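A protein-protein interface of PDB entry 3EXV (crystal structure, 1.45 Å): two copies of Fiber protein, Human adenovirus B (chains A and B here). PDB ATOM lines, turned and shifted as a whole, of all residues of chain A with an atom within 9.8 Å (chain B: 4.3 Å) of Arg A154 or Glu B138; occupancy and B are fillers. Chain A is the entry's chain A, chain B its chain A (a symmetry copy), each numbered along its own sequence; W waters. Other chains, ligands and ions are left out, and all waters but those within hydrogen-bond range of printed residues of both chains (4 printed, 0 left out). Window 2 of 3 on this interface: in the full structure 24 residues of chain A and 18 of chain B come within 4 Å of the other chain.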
ATOM      1  N   TYR A  62      -8.179 -25.882 -16.123  1.00  0.00           N
ATOM      2  CA  TYR A  62      -9.197 -25.202 -15.318  1.00  0.00           C
ATOM      3  C   TYR A  62     -10.570 -25.816 -15.539  1.00  0.00           C
ATOM      4  O   TYR A  62     -10.745 -26.672 -16.408  1.00  0.00           O
ATOM      5  CB  TYR A  62      -9.230 -23.692 -15.596  1.00  0.00           C
ATOM      6  CG  TYR A  62      -9.567 -23.286 -17.017  1.00  0.00           C
ATOM      7  CD1 TYR A  62      -8.623 -23.387 -18.033  1.00  0.00           C
ATOM      8  CD2 TYR A  62     -10.812 -22.740 -17.332  1.00  0.00           C
ATOM      9  CE1 TYR A  62      -8.918 -22.990 -19.332  1.00  0.00           C
ATOM     10  CE2 TYR A  62     -11.115 -22.338 -18.632  1.00  0.00           C
ATOM     11  CZ  TYR A  62     -10.164 -22.466 -19.625  1.00  0.00           C
ATOM     12  OH  TYR A  62     -10.452 -22.066 -20.914  1.00  0.00           O
ATOM     13  N   ILE A  64     -14.901 -25.059 -15.846  1.00  0.00           N
ATOM     14  CA  ILE A  64     -16.041 -24.175 -16.030  1.00  0.00           C
ATOM     15  C   ILE A  64     -17.271 -24.930 -15.544  1.00  0.00           C
ATOM     16  O   ILE A  64     -17.674 -25.920 -16.149  1.00  0.00           O
ATOM     17  CB  ILE A  64     -16.232 -23.791 -17.512  1.00  0.00           C
ATOM     18  CG1 ILE A  64     -14.975 -23.112 -18.062  1.00  0.00           C
ATOM     19  CG2 ILE A  64     -17.438 -22.874 -17.673  1.00  0.00           C
ATOM     20  CD1 ILE A  64     -14.957 -23.001 -19.578  1.00  0.00           C
ATOM     21  N   TYR A 148      -7.354 -19.117  -9.021  1.00  0.00           N
ATOM     22  CA  TYR A 148      -8.273 -18.141  -8.449  1.00  0.00           C
ATOM     23  C   TYR A 148      -9.678 -18.227  -9.015  1.00  0.00           C
ATOM     24  O   TYR A 148      -9.871 -18.464 -10.208  1.00  0.00           O
ATOM     25  CB  TYR A 148      -7.724 -16.726  -8.658  1.00  0.00           C
ATOM     26  CG  TYR A 148      -6.357 -16.521  -8.052  1.00  0.00           C
ATOM     27  CD1 TYR A 148      -5.206 -16.898  -8.739  1.00  0.00           C
ATOM     28  CD2 TYR A 148      -6.213 -15.975  -6.782  1.00  0.00           C
ATOM     29  CE1 TYR A 148      -3.948 -16.727  -8.181  1.00  0.00           C
ATOM     30  CE2 TYR A 148      -4.958 -15.799  -6.214  1.00  0.00           C
ATOM     31  CZ  TYR A 148      -3.830 -16.174  -6.920  1.00  0.00           C
ATOM     32  OH  TYR A 148      -2.583 -16.000  -6.362  1.00  0.00           O
ATOM     33  N   TYR A 149     -10.654 -18.041  -8.133  1.00  0.00           N
ATOM     34  CA  TYR A 149     -12.040 -17.865  -8.525  1.00  0.00           C
ATOM     35  C   TYR A 149     -12.339 -16.372  -8.537  1.00  0.00           C
ATOM     36  O   TYR A 149     -12.075 -15.680  -7.557  1.00  0.00           O
ATOM     37  CB  TYR A 149     -12.973 -18.580  -7.540  1.00  0.00           C
ATOM     38  CG  TYR A 149     -14.414 -18.131  -7.635  1.00  0.00           C
ATOM     39  CD1 TYR A 149     -15.195 -18.475  -8.731  1.00  0.00           C
ATOM     40  CD2 TYR A 149     -14.989 -17.350  -6.637  1.00  0.00           C
ATOM     41  CE1 TYR A 149     -16.509 -18.059  -8.833  1.00  0.00           C
ATOM     42  CE2 TYR A 149     -16.309 -16.930  -6.729  1.00  0.00           C
ATOM     43  CZ  TYR A 149     -17.063 -17.286  -7.831  1.00  0.00           C
ATOM     44  OH  TYR A 149     -18.369 -16.869  -7.940  1.00  0.00           O
ATOM     45  N   THR A 150     -12.859 -15.874  -9.655  1.00  0.00           N
ATOM     46  CA  THR A 150     -13.247 -14.471  -9.756  1.00  0.00           C
ATOM     47  C   THR A 150     -14.638 -14.309  -9.159  1.00  0.00           C
ATOM     48  O   THR A 150     -15.629 -14.726  -9.756  1.00  0.00           O
ATOM     49  CB  THR A 150     -13.238 -13.978 -11.220  1.00  0.00           C
ATOM     50  OG1 THR A 150     -11.919 -14.115 -11.762  1.00  0.00           O
ATOM     51  CG2 THR A 150     -13.662 -12.514 -11.301  1.00  0.00           C
ATOM     52  N   ALA A 151     -14.702 -13.716  -7.970  1.00  0.00           N
ATOM     53  CA  ALA A 151     -15.965 -13.571  -7.252  1.00  0.00           C
ATOM     54  C   ALA A 151     -16.853 -12.505  -7.885  1.00  0.00           C
ATOM     55  O   ALA A 151     -16.412 -11.744  -8.748  1.00  0.00           O
ATOM     56  CB  ALA A 151     -15.706 -13.244  -5.788  1.00  0.00           C
ATOM     57  N   SER A 152     -18.104 -12.453  -7.440  1.00  0.00           N
ATOM     58  CA  SER A 152     -19.079 -11.497  -7.969  1.00  0.00           C
ATOM     59  C   SER A 152     -18.633 -10.047  -7.763  1.00  0.00           C
ATOM     60  O   SER A 152     -19.000  -9.170  -8.542  1.00  0.00           O
ATOM     61  CB  SER A 152     -20.452 -11.722  -7.329  1.00  0.00           C
ATOM     62  OG  SER A 152     -20.362 -11.724  -5.919  1.00  0.00           O
ATOM     63  N   ASP A 153     -17.832  -9.804  -6.726  1.00  0.00           N
ATOM     64  CA  ASP A 153     -17.271  -8.468  -6.482  1.00  0.00           C
ATOM     65  C   ASP A 153     -15.925  -8.254  -7.204  1.00  0.00           C
ATOM     66  O   ASP A 153     -15.224  -7.271  -6.945  1.00  0.00           O
ATOM     67  CB  ASP A 153     -17.123  -8.209  -4.975  1.00  0.00           C
ATOM     68  CG  ASP A 153     -15.991  -9.004  -4.343  1.00  0.00           C
ATOM     69  OD1 ASP A 153     -15.581  -8.644  -3.219  1.00  0.00           O
ATOM     70  OD2 ASP A 153     -15.511  -9.981  -4.959  1.00  0.00           O
ATOM     71  N   ARG A 154     -15.580  -9.187  -8.097  1.00  0.00           N
ATOM     72  CA  ARG A 154     -14.362  -9.122  -8.932  1.00  0.00           C
ATOM     73  C   ARG A 154     -13.038  -9.296  -8.172  1.00  0.00           C
ATOM     74  O   ARG A 154     -11.964  -9.111  -8.750  1.00  0.00           O
ATOM     75  CB  ARG A 154     -14.338  -7.839  -9.791  1.00  0.00           C
ATOM     76  CG  ARG A 154     -15.046  -7.987 -11.138  1.00  0.00           C
ATOM     77  CD  ARG A 154     -16.528  -8.273 -10.963  1.00  0.00           C
ATOM     78  NE  ARG A 154     -17.251  -8.265 -12.237  1.00  0.00           N
ATOM     79  CZ  ARG A 154     -17.604  -7.166 -12.904  1.00  0.00           C
ATOM     80  NH1 ARG A 154     -17.287  -5.965 -12.440  1.00  0.00           N
ATOM     81  NH2 ARG A 154     -18.269  -7.272 -14.050  1.00  0.00           N
ATOM     82  N   THR A 155     -13.108  -9.684  -6.900  1.00  0.00           N
ATOM     83  CA  THR A 155     -11.900 -10.012  -6.146  1.00  0.00           C
ATOM     84  C   THR A 155     -11.428 -11.410  -6.535  1.00  0.00           C
ATOM     85  O   THR A 155     -12.238 -12.271  -6.895  1.00  0.00           O
ATOM     86  CB  THR A 155     -12.131  -9.960  -4.622  1.00  0.00           C
ATOM     87  OG1 THR A 155     -13.145 -10.901  -4.252  1.00  0.00           O
ATOM     88  CG2 THR A 155     -12.549  -8.560  -4.186  1.00  0.00           C
ATOM     89  N   ALA A 156     -10.117 -11.624  -6.478  1.00  0.00           N
ATOM     90  CA  ALA A 156      -9.531 -12.920  -6.807  1.00  0.00           C
ATOM     91  C   ALA A 156      -9.451 -13.792  -5.558  1.00  0.00           C
ATOM     92  O   ALA A 156      -8.636 -13.549  -4.666  1.00  0.00           O
ATOM     93  CB  ALA A 156      -8.149 -12.737  -7.417  1.00  0.00           C
ATOM     94  N   PHE A 157     -10.314 -14.803  -5.499  1.00  0.00           N
ATOM     95  CA  PHE A 157     -10.379 -15.714  -4.361  1.00  0.00           C
ATOM     96  C   PHE A 157      -9.404 -16.872  -4.579  1.00  0.00           C
ATOM     97  O   PHE A 157      -9.574 -17.653  -5.513  1.00  0.00           O
ATOM     98  CB  PHE A 157     -11.807 -16.246  -4.207  1.00  0.00           C
ATOM     99  CG  PHE A 157     -11.977 -17.226  -3.084  1.00  0.00           C
ATOM    100  CD1 PHE A 157     -12.232 -16.786  -1.794  1.00  0.00           C
ATOM    101  CD2 PHE A 157     -11.906 -18.592  -3.324  1.00  0.00           C
ATOM    102  CE1 PHE A 157     -12.399 -17.695  -0.755  1.00  0.00           C
ATOM    103  CE2 PHE A 157     -12.072 -19.502  -2.293  1.00  0.00           C
ATOM    104  CZ  PHE A 157     -12.321 -19.055  -1.007  1.00  0.00           C
ATOM    105  N   PRO A 190     -16.602 -17.525  -0.736  1.00  0.00           N
ATOM    106  CA  PRO A 190     -16.476 -16.427  -1.703  1.00  0.00           C
ATOM    107  C   PRO A 190     -17.814 -15.815  -2.131  1.00  0.00           C
ATOM    108  O   PRO A 190     -17.850 -14.658  -2.555  1.00  0.00           O
ATOM    109  CB  PRO A 190     -15.777 -17.085  -2.902  1.00  0.00           C
ATOM    110  CG  PRO A 190     -16.021 -18.531  -2.758  1.00  0.00           C
ATOM    111  CD  PRO A 190     -16.133 -18.807  -1.292  1.00  0.00           C
ATOM    112  N   GLU A 191     -18.896 -16.588  -2.028  1.00  0.00           N
ATOM    113  CA  GLU A 191     -20.220 -16.119  -2.433  1.00  0.00           C
ATOM    114  C   GLU A 191     -21.287 -16.446  -1.402  1.00  0.00           C
ATOM    115  O   GLU A 191     -21.091 -17.293  -0.529  1.00  0.00           O
ATOM    116  CB  GLU A 191     -20.629 -16.765  -3.761  1.00  0.00           C
ATOM    117  CG  GLU A 191     -19.675 -16.521  -4.919  1.00  0.00           C
ATOM    118  CD  GLU A 191     -19.716 -15.097  -5.446  1.00  0.00           C
ATOM    119  OE1 GLU A 191     -20.484 -14.266  -4.915  1.00  0.00           O
ATOM    120  OE2 GLU A 191     -18.975 -14.810  -6.406  1.00  0.00           O
ATOM    121  N   SER A 195     -25.638 -14.229  -4.629  1.00  0.00           N
ATOM    122  CA  SER A 195     -24.588 -13.677  -5.499  1.00  0.00           C
ATOM    123  C   SER A 195     -23.895 -14.736  -6.370  1.00  0.00           C
ATOM    124  O   SER A 195     -23.192 -14.393  -7.321  1.00  0.00           O
ATOM    125  CB  SER A 195     -23.538 -12.954  -4.654  1.00  0.00           C
ATOM    126  OG  SER A 195     -22.902 -13.847  -3.754  1.00  0.00           O
ATOM    127  N   THR A 197     -23.056 -17.570  -9.106  1.00  0.00           N
ATOM    128  CA  THR A 197     -23.443 -17.814 -10.498  1.00  0.00           C
ATOM    129  C   THR A 197     -22.792 -19.093 -11.035  1.00  0.00           C
ATOM    130  O   THR A 197     -23.407 -20.158 -11.020  1.00  0.00           O
ATOM    131  CB  THR A 197     -23.071 -16.621 -11.412  1.00  0.00           C
ATOM    132  OG1 THR A 197     -21.676 -16.324 -11.279  1.00  0.00           O
ATOM    133  CG2 THR A 197     -23.888 -15.389 -11.049  1.00  0.00           C
ATOM    134  N   THR A 198     -21.549 -18.979 -11.501  1.00  0.00           N
ATOM    135  CA  THR A 198     -20.826 -20.110 -12.083  1.00  0.00           C
ATOM    136  C   THR A 198     -19.465 -20.272 -11.416  1.00  0.00           C
ATOM    137  O   THR A 198     -18.721 -19.301 -11.267  1.00  0.00           O
ATOM    138  CB  THR A 198     -20.606 -19.915 -13.601  1.00  0.00           C
ATOM    139  OG1 THR A 198     -21.871 -19.772 -14.261  1.00  0.00           O
ATOM    140  CG2 THR A 198     -19.856 -21.101 -14.197  1.00  0.00           C
ATOM    141  N   VAL A 200     -16.003 -20.987 -11.842  1.00  0.00           N
ATOM    142  CA  VAL A 200     -14.932 -21.051 -12.827  1.00  0.00           C
ATOM    143  C   VAL A 200     -13.607 -20.834 -12.116  1.00  0.00           C
ATOM    144  O   VAL A 200     -13.497 -19.954 -11.270  1.00  0.00           O
ATOM    145  CB  VAL A 200     -15.100 -19.967 -13.912  1.00  0.00           C
ATOM    146  CG1 VAL A 200     -13.927 -19.994 -14.888  1.00  0.00           C
ATOM    147  CG2 VAL A 200     -16.419 -20.150 -14.647  1.00  0.00           C
ATOM    148  N   THR A 201     -12.608 -21.651 -12.441  1.00  0.00           N
ATOM    149  CA  THR A 201     -11.266 -21.456 -11.900  1.00  0.00           C
ATOM    150  C   THR A 201     -10.367 -20.850 -12.969  1.00  0.00           C
ATOM    151  O   THR A 201     -10.530 -21.129 -14.158  1.00  0.00           O
ATOM    152  CB  THR A 201     -10.646 -22.776 -11.386  1.00  0.00           C
ATOM    153  OG1 THR A 201     -10.504 -23.705 -12.467  1.00  0.00           O
ATOM    154  CG2 THR A 201     -11.516 -23.390 -10.295  1.00  0.00           C
ATOM    155  N   SER A 202      -9.435 -20.002 -12.548  1.00  0.00           N
ATOM    156  CA  SER A 202      -8.468 -19.422 -13.472  1.00  0.00           C
ATOM    157  C   SER A 202      -7.470 -20.507 -13.877  1.00  0.00           C
ATOM    158  O   SER A 202      -7.200 -21.420 -13.096  1.00  0.00           O
ATOM    159  CB  SER A 202      -7.748 -18.225 -12.839  1.00  0.00           C
ATOM    160  OG  SER A 202      -6.903 -18.623 -11.775  1.00  0.00           O
ATOM    161  N   PRO A 203      -6.928 -20.422 -15.104  1.00  0.00           N
ATOM    162  CA  PRO A 203      -6.025 -21.474 -15.569  1.00  0.00           C
ATOM    163  C   PRO A 203      -4.825 -21.687 -14.647  1.00  0.00           C
ATOM    164  O   PRO A 203      -4.164 -20.724 -14.251  1.00  0.00           O
ATOM    165  CB  PRO A 203      -5.567 -20.966 -16.941  1.00  0.00           C
ATOM    166  CG  PRO A 203      -6.609 -20.010 -17.365  1.00  0.00           C
ATOM    167  CD  PRO A 203      -7.116 -19.373 -16.122  1.00  0.00           C
ATOM    168  N   ASP B 134     -19.274 -10.961 -23.062  1.00  0.00           N
ATOM    169  CA  ASP B 134     -20.107 -12.082 -22.610  1.00  0.00           C
ATOM    170  C   ASP B 134     -20.109 -12.161 -21.080  1.00  0.00           C
ATOM    171  O   ASP B 134     -19.213 -12.752 -20.479  1.00  0.00           O
ATOM    172  CB  ASP B 134     -19.620 -13.399 -23.227  1.00  0.00           C
ATOM    173  CG  ASP B 134     -20.628 -14.530 -23.071  1.00  0.00           C
ATOM    174  OD1 ASP B 134     -21.431 -14.496 -22.115  1.00  0.00           O
ATOM    175  OD2 ASP B 134     -20.610 -15.459 -23.905  1.00  0.00           O
ATOM    176  N   ASN B 135     -21.125 -11.561 -20.461  1.00  0.00           N
ATOM    177  CA  ASN B 135     -21.229 -11.523 -18.997  1.00  0.00           C
ATOM    178  C   ASN B 135     -21.332 -12.916 -18.375  1.00  0.00           C
ATOM    179  O   ASN B 135     -20.801 -13.156 -17.289  1.00  0.00           O
ATOM    180  CB  ASN B 135     -22.433 -10.677 -18.560  1.00  0.00           C
ATOM    181  CG  ASN B 135     -22.252  -9.200 -18.862  1.00  0.00           C
ATOM    182  OD1 ASN B 135     -21.489  -8.821 -19.753  1.00  0.00           O
ATOM    183  ND2 ASN B 135     -22.966  -8.355 -18.123  1.00  0.00           N
ATOM    184  N   SER B 136     -22.009 -13.829 -19.068  1.00  0.00           N
ATOM    185  CA  SER B 136     -22.188 -15.196 -18.573  1.00  0.00           C
ATOM    186  C   SER B 136     -20.883 -16.003 -18.591  1.00  0.00           C
ATOM    187  O   SER B 136     -20.777 -17.029 -17.917  1.00  0.00           O
ATOM    188  CB  SER B 136     -23.264 -15.926 -19.387  1.00  0.00           C
ATOM    189  OG  SER B 136     -22.840 -16.159 -20.718  1.00  0.00           O
ATOM    190  N   ARG B 137     -19.900 -15.543 -19.369  1.00  0.00           N
ATOM    191  CA  ARG B 137     -18.599 -16.211 -19.465  1.00  0.00           C
ATOM    192  C   ARG B 137     -17.445 -15.334 -18.962  1.00  0.00           C
ATOM    193  O   ARG B 137     -16.280 -15.683 -19.146  1.00  0.00           O
ATOM    194  CB  ARG B 137     -18.318 -16.607 -20.916  1.00  0.00           C
ATOM    195  CG  ARG B 137     -19.211 -17.703 -21.468  1.00  0.00           C
ATOM    196  CD  ARG B 137     -18.779 -18.089 -22.876  1.00  0.00           C
ATOM    197  NE  ARG B 137     -17.412 -18.612 -22.892  1.00  0.00           N
ATOM    198  CZ  ARG B 137     -16.655 -18.741 -23.980  1.00  0.00           C
ATOM    199  NH1 ARG B 137     -17.109 -18.383 -25.178  1.00  0.00           N
ATOM    200  NH2 ARG B 137     -15.425 -19.227 -23.864  1.00  0.00           N
ATOM    201  N   GLU B 138     -17.765 -14.218 -18.306  1.00  0.00           N
ATOM    202  CA  GLU B 138     -16.749 -13.207 -17.975  1.00  0.00           C
ATOM    203  C   GLU B 138     -15.607 -13.732 -17.099  1.00  0.00           C
ATOM    204  O   GLU B 138     -14.474 -13.264 -17.214  1.00  0.00           O
ATOM    205  CB  GLU B 138     -17.389 -11.980 -17.309  1.00  0.00           C
ATOM    206  CG  GLU B 138     -17.887 -12.201 -15.877  1.00  0.00           C
ATOM    207  CD  GLU B 138     -18.053 -10.903 -15.105  1.00  0.00           C
ATOM    208  OE1 GLU B 138     -17.864  -9.821 -15.698  1.00  0.00           O
ATOM    209  OE2 GLU B 138     -18.359 -10.968 -13.896  1.00  0.00           O
ATOM    210  N   LYS B 139     -15.902 -14.699 -16.232  1.00  0.00           N
ATOM    211  CA  LYS B 139     -14.885 -15.244 -15.323  1.00  0.00           C
ATOM    212  C   LYS B 139     -13.753 -15.927 -16.093  1.00  0.00           C
ATOM    213  O   LYS B 139     -12.623 -15.996 -15.612  1.00  0.00           O
ATOM    214  CB  LYS B 139     -15.512 -16.226 -14.327  1.00  0.00           C
ATOM    215  CG  LYS B 139     -16.534 -15.593 -13.386  1.00  0.00           C
ATOM    216  CD  LYS B 139     -16.993 -16.574 -12.312  1.00  0.00           C
ATOM    217  CE  LYS B 139     -18.255 -16.091 -11.610  1.00  0.00           C
ATOM    218  NZ  LYS B 139     -18.077 -14.767 -10.959  1.00  0.00           N
ATOM    219  N   GLU B 140     -14.059 -16.405 -17.300  1.00  0.00           N
ATOM    220  CA  GLU B 140     -13.072 -17.086 -18.141  1.00  0.00           C
ATOM    221  C   GLU B 140     -12.033 -16.129 -18.742  1.00  0.00           C
ATOM    222  O   GLU B 140     -10.992 -16.569 -19.225  1.00  0.00           O
ATOM    223  CB  GLU B 140     -13.776 -17.846 -19.268  1.00  0.00           C
ATOM    224  CG  GLU B 140     -14.724 -18.929 -18.781  1.00  0.00           C
ATOM    225  CD  GLU B 140     -15.535 -19.539 -19.902  1.00  0.00           C
ATOM    226  OE1 GLU B 140     -14.938 -19.912 -20.933  1.00  0.00           O
ATOM    227  OE2 GLU B 140     -16.770 -19.655 -19.750  1.00  0.00           O
ATOM    228  N   ASN B 141     -12.319 -14.829 -18.708  1.00  0.00           N
ATOM    229  CA  ASN B 141     -11.428 -13.825 -19.297  1.00  0.00           C
ATOM    230  C   ASN B 141     -10.251 -13.437 -18.398  1.00  0.00           C
ATOM    231  O   ASN B 141      -9.407 -12.638 -18.801  1.00  0.00           O
ATOM    232  CB  ASN B 141     -12.222 -12.562 -19.647  1.00  0.00           C
ATOM    233  CG  ASN B 141     -13.228 -12.791 -20.753  1.00  0.00           C
ATOM    234  OD1 ASN B 141     -14.413 -13.002 -20.495  1.00  0.00           O
ATOM    235  ND2 ASN B 141     -12.762 -12.756 -21.995  1.00  0.00           N
ATOM    236  N   TYR B 142     -10.182 -14.013 -17.196  1.00  0.00           N
ATOM    237  CA  TYR B 142      -9.227 -13.561 -16.180  1.00  0.00           C
ATOM    238  C   TYR B 142      -8.130 -14.568 -15.843  1.00  0.00           C
ATOM    239  O   TYR B 142      -8.393 -15.758 -15.662  1.00  0.00           O
ATOM    240  CB  TYR B 142      -9.970 -13.204 -14.896  1.00  0.00           C
ATOM    241  CG  TYR B 142     -10.777 -11.936 -14.984  1.00  0.00           C
ATOM    242  CD1 TYR B 142     -12.118 -11.967 -15.354  1.00  0.00           C
ATOM    243  CD2 TYR B 142     -10.208 -10.705 -14.680  1.00  0.00           C
ATOM    244  CE1 TYR B 142     -12.868 -10.802 -15.424  1.00  0.00           C
ATOM    245  CE2 TYR B 142     -10.949  -9.536 -14.746  1.00  0.00           C
ATOM    246  CZ  TYR B 142     -12.277  -9.590 -15.122  1.00  0.00           C
ATOM    247  OH  TYR B 142     -13.017  -8.433 -15.184  1.00  0.00           O
ATOM    248  N   ARG B 167     -12.610  -9.537 -23.696  1.00  0.00           N
ATOM    249  CA  ARG B 167     -13.677  -9.086 -22.767  1.00  0.00           C
ATOM    250  C   ARG B 167     -14.317  -7.742 -23.138  1.00  0.00           C
ATOM    251  O   ARG B 167     -15.534  -7.660 -23.308  1.00  0.00           O
ATOM    252  CB  ARG B 167     -13.159  -9.028 -21.320  1.00  0.00           C
ATOM    253  CG  ARG B 167     -14.207  -8.614 -20.287  1.00  0.00           C
ATOM    254  CD  ARG B 167     -15.237  -9.693 -20.058  1.00  0.00           C
ATOM    255  NE  ARG B 167     -16.264  -9.261 -19.106  1.00  0.00           N
ATOM    256  CZ  ARG B 167     -17.503  -8.884 -19.427  1.00  0.00           C
ATOM    257  NH1 ARG B 167     -17.920  -8.893 -20.688  1.00  0.00           N
ATOM    258  NH2 ARG B 167     -18.342  -8.509 -18.470  1.00  0.00           N
HETATM  259  O   HOH W   1     -12.384 -20.339 -21.712  1.00  0.00           O
HETATM  260  O   HOH W   2     -22.205 -17.291 -15.537  1.00  0.00           O
HETATM  261  O   HOH W   3     -17.449 -12.190 -11.634  1.00  0.00           O
HETATM  262  O   HOH W   4     -20.733 -14.643  -9.390  1.00  0.00           O
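Of chain B, only Glu B138 (3.1 Å) comes within 4 Å of Arg A154.
Of chain A, only Arg A154 (3.1 Å) comes within 4 Å of Glu B138.
Printed residues of chain A within 4 Å of Glu B140: Ile A64.
Printed residues of chain B within 4 Å of Ser A202: Tyr B142.
Of the printed residues of chain B, Thr A198 touches Lys B139.
Asp A153 touches none of the printed residues of chain B.
Ser A195 touches none of the printed residues of chain B.
The nearest printed residue of chain B that does not touch Arg A154 is Tyr B142 (4.5 Å).
The nearest printed residue of chain A that does not touch Glu B138 is Ala A151 (5.6 Å).
N of Tyr A148 lies within hydrogen-bond range of OG of Ser A202 (2.8 Å).
O of Tyr A149 lies within hydrogen-bond range of N of Phe A157.
OH of Tyr A149 is in hydrogen-bond range of OE2 of Glu A191 (2.6 Å).
NH2 of Arg B137 lies within salt-bridge range of OE1 of Glu B140 (3.0 Å).
OD1 of Asn B141 sits close to O of Glu B138 (3.3 Å).
OE1 of Glu B138 lies within salt-bridge range of NH2 of Arg B167.
Among the printed residues, pairs that only touch across the chains: Thr A198 with Lys B139 (3.3 Å), Ile A64 with Glu B140 (3.4 Å), Thr A197 with Lys B139 (3.4 Å), Tyr A149 with Lys B139 (3.7 Å), Val A200 with Lys B139 (3.8 Å), Thr A150 with Tyr B142 (3.8 Å), Ser A202 with Tyr B142 (3.8 Å) and Pro A203 with Tyr B142 (3.9 Å).
O of Thr A150 sits at hydrogen-bond distance from NZ of Lys B139 (2.7 Å).
The guanidinium group (NH2) of Arg A154 is in salt-bridge range of the side-chain carboxylate (OE1) of Glu B138, at 3.1 Å.
No position is printed for both chains.
Of the 10 pairs that touch across the chains among the printed residues, none has its exchanged pair printed and touching as well.
Of the 21 printed residues of chain A, 9 touch a printed residue of chain B.
Printed residues of chain B that touch a printed residue of chain A: Glu B138, Lys B139, Glu B140 and Tyr B142.
Among the printed residues, Asp or Glu carboxylates within 4 Å of a Lys or Arg side-chain nitrogen of the other chain: Arg A154 with Glu B138 (3.1 Å).
Water W4 lies within hydrogen-bond range of OG1 of Thr A197 (2.7 Å), NZ of Lys B139 (3.1 Å), O of Ser A195 (3.2 Å) and OE2 of Glu A191 (3.5 Å).
Water W1 lies within hydrogen-bond range of OE1 of Glu B140 (2.7 Å) and OH of Tyr A62 (2.7 Å).
Water W3 lies within hydrogen-bond range of the side-chain carboxylate (OE2) of Glu B138 (2.7 Å), the side-chain amino group (NZ) of Lys B139 (2.7 Å) and the backbone carbonyl oxygen (O) of Ala A151 (3.1 Å).
Water W2 bridges the backbone carbonyl oxygen of Ser B136 (2.8 Å) and the side-chain hydroxyl of Thr A198 (2.8 Å).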
